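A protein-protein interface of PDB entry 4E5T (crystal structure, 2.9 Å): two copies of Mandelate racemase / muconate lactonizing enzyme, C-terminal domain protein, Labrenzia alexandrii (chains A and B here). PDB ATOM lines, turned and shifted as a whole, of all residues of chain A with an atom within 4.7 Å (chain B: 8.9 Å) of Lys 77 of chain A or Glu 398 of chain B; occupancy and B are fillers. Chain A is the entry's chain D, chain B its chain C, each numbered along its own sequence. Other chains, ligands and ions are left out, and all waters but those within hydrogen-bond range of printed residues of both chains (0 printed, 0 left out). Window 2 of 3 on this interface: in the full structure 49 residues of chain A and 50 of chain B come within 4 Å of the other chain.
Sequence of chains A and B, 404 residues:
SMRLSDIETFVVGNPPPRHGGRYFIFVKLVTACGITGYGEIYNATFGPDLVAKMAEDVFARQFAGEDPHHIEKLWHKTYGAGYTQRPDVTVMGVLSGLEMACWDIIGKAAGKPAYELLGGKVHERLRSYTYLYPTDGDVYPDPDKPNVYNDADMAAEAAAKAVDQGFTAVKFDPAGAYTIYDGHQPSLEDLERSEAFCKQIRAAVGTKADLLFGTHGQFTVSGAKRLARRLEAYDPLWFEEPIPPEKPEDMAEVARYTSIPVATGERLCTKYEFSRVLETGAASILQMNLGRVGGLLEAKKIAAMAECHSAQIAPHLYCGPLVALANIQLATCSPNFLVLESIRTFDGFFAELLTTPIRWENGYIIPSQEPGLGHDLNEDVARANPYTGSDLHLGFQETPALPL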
ATOM      1  N   ARG A  61      14.580 -10.142 -25.741  1.00  0.00           N
ATOM      2  CA  ARG A  61      15.322  -9.017 -26.313  1.00  0.00           C
ATOM      3  C   ARG A  61      15.211  -7.698 -25.545  1.00  0.00           C
ATOM      4  O   ARG A  61      16.096  -6.849 -25.631  1.00  0.00           O
ATOM      5  CB  ARG A  61      14.897  -8.769 -27.755  1.00  0.00           C
ATOM      6  CG  ARG A  61      15.435  -9.756 -28.759  1.00  0.00           C
ATOM      7  CD  ARG A  61      15.286  -9.193 -30.168  1.00  0.00           C
ATOM      8  NE  ARG A  61      15.234 -10.236 -31.188  1.00  0.00           N
ATOM      9  CZ  ARG A  61      16.302 -10.846 -31.694  1.00  0.00           C
ATOM     10  NH1 ARG A  61      17.510 -10.527 -31.261  1.00  0.00           N
ATOM     11  NH2 ARG A  61      16.163 -11.779 -32.628  1.00  0.00           N
ATOM     12  N   GLN A  62      14.123  -7.511 -24.808  1.00  0.00           N
ATOM     13  CA  GLN A  62      13.876  -6.216 -24.192  1.00  0.00           C
ATOM     14  C   GLN A  62      13.627  -6.290 -22.683  1.00  0.00           C
ATOM     15  O   GLN A  62      13.933  -5.349 -21.951  1.00  0.00           O
ATOM     16  CB  GLN A  62      12.700  -5.525 -24.890  1.00  0.00           C
ATOM     17  CG  GLN A  62      12.659  -5.691 -26.409  1.00  0.00           C
ATOM     18  CD  GLN A  62      13.730  -4.885 -27.136  1.00  0.00           C
ATOM     19  OE1 GLN A  62      14.396  -4.017 -26.554  1.00  0.00           O
ATOM     20  NE2 GLN A  62      13.898  -5.171 -28.425  1.00  0.00           N
ATOM     21  N   GLU A  66      15.570  -6.514 -16.900  1.00  0.00           N
ATOM     22  CA  GLU A  66      15.062  -5.197 -16.563  1.00  0.00           C
ATOM     23  C   GLU A  66      14.125  -5.266 -15.370  1.00  0.00           C
ATOM     24  O   GLU A  66      13.557  -6.316 -15.066  1.00  0.00           O
ATOM     25  CB  GLU A  66      14.349  -4.556 -17.759  1.00  0.00           C
ATOM     26  CG  GLU A  66      15.258  -4.156 -18.917  1.00  0.00           C
ATOM     27  CD  GLU A  66      16.014  -2.847 -18.680  1.00  0.00           C
ATOM     28  OE1 GLU A  66      15.793  -2.194 -17.627  1.00  0.00           O
ATOM     29  OE2 GLU A  66      16.834  -2.481 -19.560  1.00  0.00           O
ATOM     30  N   LYS A  73      10.679   2.669 -20.272  1.00  0.00           N
ATOM     31  CA  LYS A  73      11.900   2.160 -20.884  1.00  0.00           C
ATOM     32  C   LYS A  73      11.575   0.918 -21.699  1.00  0.00           C
ATOM     33  O   LYS A  73      11.894   0.846 -22.888  1.00  0.00           O
ATOM     34  CB  LYS A  73      12.946   1.830 -19.821  1.00  0.00           C
ATOM     35  CG  LYS A  73      14.290   1.328 -20.346  1.00  0.00           C
ATOM     36  CD  LYS A  73      15.168   0.961 -19.157  1.00  0.00           C
ATOM     37  CE  LYS A  73      16.663   1.064 -19.436  1.00  0.00           C
ATOM     38  NZ  LYS A  73      17.435   0.841 -18.173  1.00  0.00           N
ATOM     39  N   LEU A  74      10.925  -0.050 -21.061  1.00  0.00           N
ATOM     40  CA  LEU A  74      10.563  -1.288 -21.739  1.00  0.00           C
ATOM     41  C   LEU A  74       9.673  -1.029 -22.957  1.00  0.00           C
ATOM     42  O   LEU A  74       9.912  -1.571 -24.040  1.00  0.00           O
ATOM     43  CB  LEU A  74       9.872  -2.248 -20.771  1.00  0.00           C
ATOM     44  CG  LEU A  74      10.736  -2.880 -19.682  1.00  0.00           C
ATOM     45  CD1 LEU A  74       9.827  -3.416 -18.605  1.00  0.00           C
ATOM     46  CD2 LEU A  74      11.611  -3.996 -20.240  1.00  0.00           C
ATOM     47  N   TRP A  75       8.656  -0.192 -22.775  1.00  0.00           N
ATOM     48  CA  TRP A  75       7.728   0.116 -23.854  1.00  0.00           C
ATOM     49  C   TRP A  75       8.474   0.689 -25.061  1.00  0.00           C
ATOM     50  O   TRP A  75       8.281   0.239 -26.194  1.00  0.00           O
ATOM     51  CB  TRP A  75       6.640   1.089 -23.381  1.00  0.00           C
ATOM     52  CG  TRP A  75       5.430   1.057 -24.244  1.00  0.00           C
ATOM     53  CD1 TRP A  75       4.360   0.228 -24.118  1.00  0.00           C
ATOM     54  CD2 TRP A  75       5.170   1.879 -25.385  1.00  0.00           C
ATOM     55  NE1 TRP A  75       3.441   0.482 -25.103  1.00  0.00           N
ATOM     56  CE2 TRP A  75       3.914   1.494 -25.897  1.00  0.00           C
ATOM     57  CE3 TRP A  75       5.877   2.900 -26.025  1.00  0.00           C
ATOM     58  CZ2 TRP A  75       3.351   2.094 -27.027  1.00  0.00           C
ATOM     59  CZ3 TRP A  75       5.312   3.496 -27.141  1.00  0.00           C
ATOM     60  CH2 TRP A  75       4.066   3.089 -27.631  1.00  0.00           C
ATOM     61  N   HIS A  76       9.350   1.657 -24.814  1.00  0.00           N
ATOM     62  CA  HIS A  76      10.035   2.326 -25.911  1.00  0.00           C
ATOM     63  C   HIS A  76      11.142   1.499 -26.561  1.00  0.00           C
ATOM     64  O   HIS A  76      11.434   1.664 -27.746  1.00  0.00           O
ATOM     65  CB  HIS A  76      10.554   3.679 -25.461  1.00  0.00           C
ATOM     66  CG  HIS A  76       9.485   4.716 -25.348  1.00  0.00           C
ATOM     67  ND1 HIS A  76       8.927   5.081 -24.142  1.00  0.00           N
ATOM     68  CD2 HIS A  76       8.863   5.459 -26.291  1.00  0.00           C
ATOM     69  CE1 HIS A  76       8.014   6.013 -24.346  1.00  0.00           C
ATOM     70  NE2 HIS A  76       7.958   6.262 -25.642  1.00  0.00           N
ATOM     71  N   LYS A  77      11.752   0.610 -25.789  1.00  0.00           N
ATOM     72  CA  LYS A  77      12.728  -0.305 -26.347  1.00  0.00           C
ATOM     73  C   LYS A  77      12.040  -1.215 -27.354  1.00  0.00           C
ATOM     74  O   LYS A  77      12.515  -1.402 -28.468  1.00  0.00           O
ATOM     75  CB  LYS A  77      13.409  -1.120 -25.247  1.00  0.00           C
ATOM     76  CG  LYS A  77      14.483  -0.359 -24.470  1.00  0.00           C
ATOM     77  CD  LYS A  77      15.003  -1.167 -23.264  1.00  0.00           C
ATOM     78  CE  LYS A  77      15.232  -2.630 -23.636  1.00  0.00           C
ATOM     79  NZ  LYS A  77      15.951  -3.420 -22.585  1.00  0.00           N
ATOM     80  N   THR A  78      10.899  -1.756 -26.966  1.00  0.00           N
ATOM     81  CA  THR A  78      10.127  -2.623 -27.850  1.00  0.00           C
ATOM     82  C   THR A  78       9.524  -1.874 -29.028  1.00  0.00           C
ATOM     83  O   THR A  78       9.542  -2.355 -30.162  1.00  0.00           O
ATOM     84  CB  THR A  78       8.981  -3.283 -27.085  1.00  0.00           C
ATOM     85  OG1 THR A  78       9.529  -4.195 -26.122  1.00  0.00           O
ATOM     86  CG2 THR A  78       8.047  -4.022 -28.045  1.00  0.00           C
ATOM     87  N   TYR A  79       8.979  -0.700 -28.733  1.00  0.00           N
ATOM     88  CA  TYR A  79       8.335   0.137 -29.733  1.00  0.00           C
ATOM     89  C   TYR A  79       9.264   0.430 -30.888  1.00  0.00           C
ATOM     90  O   TYR A  79       8.815   0.531 -32.033  1.00  0.00           O
ATOM     91  CB  TYR A  79       7.903   1.460 -29.119  1.00  0.00           C
ATOM     92  CG  TYR A  79       7.029   2.275 -30.030  1.00  0.00           C
ATOM     93  CD1 TYR A  79       6.088   1.660 -30.851  1.00  0.00           C
ATOM     94  CD2 TYR A  79       7.117   3.661 -30.055  1.00  0.00           C
ATOM     95  CE1 TYR A  79       5.265   2.403 -31.687  1.00  0.00           C
ATOM     96  CE2 TYR A  79       6.306   4.412 -30.883  1.00  0.00           C
ATOM     97  CZ  TYR A  79       5.382   3.781 -31.699  1.00  0.00           C
ATOM     98  OH  TYR A  79       4.566   4.531 -32.513  1.00  0.00           O
ATOM     99  N   GLY A  80      10.554   0.555 -30.573  1.00  0.00           N
ATOM    100  CA  GLY A  80      11.551   0.981 -31.534  1.00  0.00           C
ATOM    101  C   GLY A  80      12.516  -0.092 -31.990  1.00  0.00           C
ATOM    102  O   GLY A  80      13.525   0.194 -32.640  1.00  0.00           O
ATOM    103  N   ALA A  81      12.214  -1.336 -31.653  1.00  0.00           N
ATOM    104  CA  ALA A  81      13.065  -2.448 -32.051  1.00  0.00           C
ATOM    105  C   ALA A  81      13.079  -2.616 -33.575  1.00  0.00           C
ATOM    106  O   ALA A  81      12.064  -2.952 -34.178  1.00  0.00           O
ATOM    107  CB  ALA A  81      12.598  -3.737 -31.365  1.00  0.00           C
ATOM    108  N   ALA B  44      12.270  -6.129 -39.541  1.00  0.00           N
ATOM    109  CA  ALA B  44      13.187  -6.334 -38.431  1.00  0.00           C
ATOM    110  C   ALA B  44      12.513  -6.159 -37.065  1.00  0.00           C
ATOM    111  O   ALA B  44      13.183  -5.956 -36.051  1.00  0.00           O
ATOM    112  CB  ALA B  44      14.360  -5.403 -38.561  1.00  0.00           C
ATOM    113  N   THR B  45      11.186  -6.238 -37.033  1.00  0.00           N
ATOM    114  CA  THR B  45      10.460  -6.094 -35.772  1.00  0.00           C
ATOM    115  C   THR B  45      10.634  -7.344 -34.906  1.00  0.00           C
ATOM    116  O   THR B  45      10.184  -7.371 -33.752  1.00  0.00           O
ATOM    117  CB  THR B  45       8.939  -5.762 -35.970  1.00  0.00           C
ATOM    118  OG1 THR B  45       8.380  -6.577 -37.009  1.00  0.00           O
ATOM    119  CG2 THR B  45       8.733  -4.301 -36.326  1.00  0.00           C
ATOM    120  N   ALA B 177      23.069  10.988 -32.620  1.00  0.00           N
ATOM    121  CA  ALA B 177      22.459   9.687 -32.387  1.00  0.00           C
ATOM    122  C   ALA B 177      20.936   9.758 -32.285  1.00  0.00           C
ATOM    123  O   ALA B 177      20.391  10.566 -31.530  1.00  0.00           O
ATOM    124  CB  ALA B 177      23.048   9.042 -31.143  1.00  0.00           C
ATOM    125  N   TYR B 178      20.255   8.918 -33.060  1.00  0.00           N
ATOM    126  CA  TYR B 178      18.815   8.782 -32.925  1.00  0.00           C
ATOM    127  C   TYR B 178      18.480   7.771 -31.843  1.00  0.00           C
ATOM    128  O   TYR B 178      19.006   6.658 -31.836  1.00  0.00           O
ATOM    129  CB  TYR B 178      18.134   8.438 -34.252  1.00  0.00           C
ATOM    130  CG  TYR B 178      18.723   7.300 -35.058  1.00  0.00           C
ATOM    131  CD1 TYR B 178      19.852   7.486 -35.854  1.00  0.00           C
ATOM    132  CD2 TYR B 178      18.114   6.054 -35.075  1.00  0.00           C
ATOM    133  CE1 TYR B 178      20.372   6.447 -36.624  1.00  0.00           C
ATOM    134  CE2 TYR B 178      18.628   5.011 -35.835  1.00  0.00           C
ATOM    135  CZ  TYR B 178      19.753   5.212 -36.609  1.00  0.00           C
ATOM    136  OH  TYR B 178      20.245   4.172 -37.365  1.00  0.00           O
ATOM    137  N   THR B 179      17.606   8.180 -30.928  1.00  0.00           N
ATOM    138  CA  THR B 179      17.347   7.435 -29.702  1.00  0.00           C
ATOM    139  C   THR B 179      15.917   6.887 -29.627  1.00  0.00           C
ATOM    140  O   THR B 179      15.047   7.268 -30.409  1.00  0.00           O
ATOM    141  CB  THR B 179      17.610   8.325 -28.470  1.00  0.00           C
ATOM    142  OG1 THR B 179      16.470   9.155 -28.210  1.00  0.00           O
ATOM    143  CG2 THR B 179      18.847   9.197 -28.690  1.00  0.00           C
ATOM    144  N   ILE B 180      15.667   5.993 -28.677  1.00  0.00           N
ATOM    145  CA  ILE B 180      14.322   5.446 -28.526  1.00  0.00           C
ATOM    146  C   ILE B 180      13.372   6.389 -27.791  1.00  0.00           C
ATOM    147  O   ILE B 180      12.246   6.011 -27.494  1.00  0.00           O
ATOM    148  CB  ILE B 180      14.320   4.094 -27.800  1.00  0.00           C
ATOM    149  CG1 ILE B 180      15.068   4.202 -26.465  1.00  0.00           C
ATOM    150  CG2 ILE B 180      14.912   3.032 -28.684  1.00  0.00           C
ATOM    151  CD1 ILE B 180      14.708   3.125 -25.466  1.00  0.00           C
ATOM    152  N   TYR B 181      13.829   7.603 -27.495  1.00  0.00           N
ATOM    153  CA  TYR B 181      12.989   8.598 -26.832  1.00  0.00           C
ATOM    154  C   TYR B 181      12.803   9.828 -27.714  1.00  0.00           C
ATOM    155  O   TYR B 181      12.373  10.886 -27.247  1.00  0.00           O
ATOM    156  CB  TYR B 181      13.585   8.993 -25.486  1.00  0.00           C
ATOM    157  CG  TYR B 181      13.651   7.847 -24.494  1.00  0.00           C
ATOM    158  CD1 TYR B 181      12.533   7.077 -24.221  1.00  0.00           C
ATOM    159  CD2 TYR B 181      14.834   7.530 -23.845  1.00  0.00           C
ATOM    160  CE1 TYR B 181      12.587   6.037 -23.320  1.00  0.00           C
ATOM    161  CE2 TYR B 181      14.894   6.488 -22.951  1.00  0.00           C
ATOM    162  CZ  TYR B 181      13.770   5.739 -22.690  1.00  0.00           C
ATOM    163  OH  TYR B 181      13.826   4.692 -21.787  1.00  0.00           O
ATOM    164  N   ASP B 182      13.143   9.673 -28.992  1.00  0.00           N
ATOM    165  CA  ASP B 182      12.894  10.688 -30.007  1.00  0.00           C
ATOM    166  C   ASP B 182      11.400  10.960 -30.122  1.00  0.00           C
ATOM    167  O   ASP B 182      10.596  10.082 -29.845  1.00  0.00           O
ATOM    168  CB  ASP B 182      13.454  10.226 -31.353  1.00  0.00           C
ATOM    169  CG  ASP B 182      14.958  10.235 -31.380  1.00  0.00           C
ATOM    170  OD1 ASP B 182      15.557  10.743 -30.402  1.00  0.00           O
ATOM    171  OD2 ASP B 182      15.532   9.744 -32.378  1.00  0.00           O
ATOM    172  N   LEU B 392      19.253  -7.482 -34.595  1.00  0.00           N
ATOM    173  CA  LEU B 392      18.259  -7.146 -35.610  1.00  0.00           C
ATOM    174  C   LEU B 392      18.879  -6.246 -36.683  1.00  0.00           C
ATOM    175  O   LEU B 392      19.892  -5.591 -36.430  1.00  0.00           O
ATOM    176  CB  LEU B 392      17.020  -6.502 -34.971  1.00  0.00           C
ATOM    177  CG  LEU B 392      16.324  -7.401 -33.940  1.00  0.00           C
ATOM    178  CD1 LEU B 392      15.052  -6.776 -33.364  1.00  0.00           C
ATOM    179  CD2 LEU B 392      16.048  -8.777 -34.542  1.00  0.00           C
ATOM    180  N   GLY B 395      18.661  -0.636 -35.531  1.00  0.00           N
ATOM    181  CA  GLY B 395      18.198  -0.311 -34.193  1.00  0.00           C
ATOM    182  C   GLY B 395      18.568   1.084 -33.722  1.00  0.00           C
ATOM    183  O   GLY B 395      19.485   1.713 -34.256  1.00  0.00           O
ATOM    184  N   PHE B 396      17.847   1.562 -32.710  1.00  0.00           N
ATOM    185  CA  PHE B 396      18.127   2.859 -32.099  1.00  0.00           C
ATOM    186  C   PHE B 396      19.235   2.799 -31.046  1.00  0.00           C
ATOM    187  O   PHE B 396      19.943   1.800 -30.899  1.00  0.00           O
ATOM    188  CB  PHE B 396      16.889   3.402 -31.386  1.00  0.00           C
ATOM    189  CG  PHE B 396      15.765   3.800 -32.291  1.00  0.00           C
ATOM    190  CD1 PHE B 396      15.654   5.102 -32.748  1.00  0.00           C
ATOM    191  CD2 PHE B 396      14.788   2.888 -32.642  1.00  0.00           C
ATOM    192  CE1 PHE B 396      14.604   5.473 -33.563  1.00  0.00           C
ATOM    193  CE2 PHE B 396      13.735   3.255 -33.456  1.00  0.00           C
ATOM    194  CZ  PHE B 396      13.646   4.545 -33.920  1.00  0.00           C
ATOM    195  N   GLN B 397      19.343   3.901 -30.307  1.00  0.00           N
ATOM    196  CA  GLN B 397      20.198   4.026 -29.136  1.00  0.00           C
ATOM    197  C   GLN B 397      19.274   4.167 -27.921  1.00  0.00           C
ATOM    198  O   GLN B 397      18.107   4.531 -28.068  1.00  0.00           O
ATOM    199  CB  GLN B 397      21.081   5.268 -29.292  1.00  0.00           C
ATOM    200  CG  GLN B 397      22.017   5.557 -28.129  1.00  0.00           C
ATOM    201  CD  GLN B 397      22.547   6.976 -28.157  1.00  0.00           C
ATOM    202  OE1 GLN B 397      21.837   7.923 -27.812  1.00  0.00           O
ATOM    203  NE2 GLN B 397      23.798   7.134 -28.580  1.00  0.00           N
ATOM    204  N   GLU B 398      19.780   3.880 -26.726  1.00  0.00           N
ATOM    205  CA  GLU B 398      18.955   3.957 -25.525  1.00  0.00           C
ATOM    206  C   GLU B 398      19.495   4.958 -24.503  1.00  0.00           C
ATOM    207  O   GLU B 398      19.264   6.164 -24.633  1.00  0.00           O
ATOM    208  CB  GLU B 398      18.799   2.566 -24.912  1.00  0.00           C
ATOM    209  CG  GLU B 398      18.391   1.510 -25.943  1.00  0.00           C
ATOM    210  CD  GLU B 398      18.688   0.083 -25.497  1.00  0.00           C
ATOM    211  OE1 GLU B 398      18.897  -0.771 -26.388  1.00  0.00           O
ATOM    212  OE2 GLU B 398      18.707  -0.187 -24.268  1.00  0.00           O
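Of the 13 printed residues of chain B, 7 touch a printed residue of chain A. Printed residues of chain B that touch a printed residue of chain A: Ala 44, Thr 45, Ile 180, Tyr 181, Leu 392, Phe 396 and Glu 398. Hydrophobic or aromatic side chains of chain B within 4 Å of the printed part of chain A: Ile 180, Tyr 181, Leu 392 and Phe 396. Along chain B the printed residues that touch a printed residue of chain A span positions 44 to 398.
Of the printed residues of chain B, His 76 of chain A touches Ile 180 and Tyr 181. Of the printed residues of chain B, Ala 81 of chain A touches Ala 44 and Thr 45. Printed residues of chain A within 4 Å of Ala 44 of chain B: Ala 81 (3.7 Å). Of the printed residues of chain A, Ile 180 of chain B touches His 76 and Lys 77. Of the printed residues of chain A, Tyr 181 of chain B touches Lys 73 and His 76. The nearest printed residue of chain A that does not touch Glu 398 of chain B is Lys 73 of chain A (5.4 Å). The nearest printed residue of chain A that does not touch Phe 396 of chain B is Ala 81 of chain A (5.0 Å).
Arg 61 of chain A touches Leu 392 of chain B. Tyr 181 of chain B touches Lys 73 of chain A. Ile 180 of chain B touches His 76 of chain A. CB of His 76 of chain A touches CE1 of Tyr 181 of chain B, 3.8 Å away. Lys 77 of chain A touches Ile 180 of chain B. Lys 77 of chain A touches Glu 398 of chain B (CD to OE2, 3.96 Å). Gly 80 of chain A touches Phe 396 of chain B. O of Ala 81 of chain A touches O of Ala 44 of chain B, 3.7 Å away. Ala 81 of chain A touches Thr 45 of chain B (O to CA, 3.9 Å).
The backbone carbonyl oxygen (O) of Gln 62 of chain A is in hydrogen-bond range of the side-chain amino group (NZ) of Lys 77 of chain A, at 2.9 Å. The side-chain hydroxyl (OG1) of Thr 179 of chain B lies close to the backbone NH (N) of Tyr 181 of chain B, 3.1 Å away. The side-chain amino group (NZ) of Lys 73 of chain A lies within salt-bridge range of the side-chain carboxylate (OE1) of Glu 66 of chain A (3.5 Å). The backbone NH (N) of Ile 180 of chain B lies within hydrogen-bond range of the backbone carbonyl oxygen (O) of Gln 397 of chain B (2.9 Å). The side-chain amino group of Lys 77 of chain A lies within salt-bridge range of the side-chain carboxylate of Glu 66 of chain A (3.3 Å).
No position is printed for both chains. Of the 9 pairs that touch across the chains among the printed residues, none has its exchanged pair printed and touching as well.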
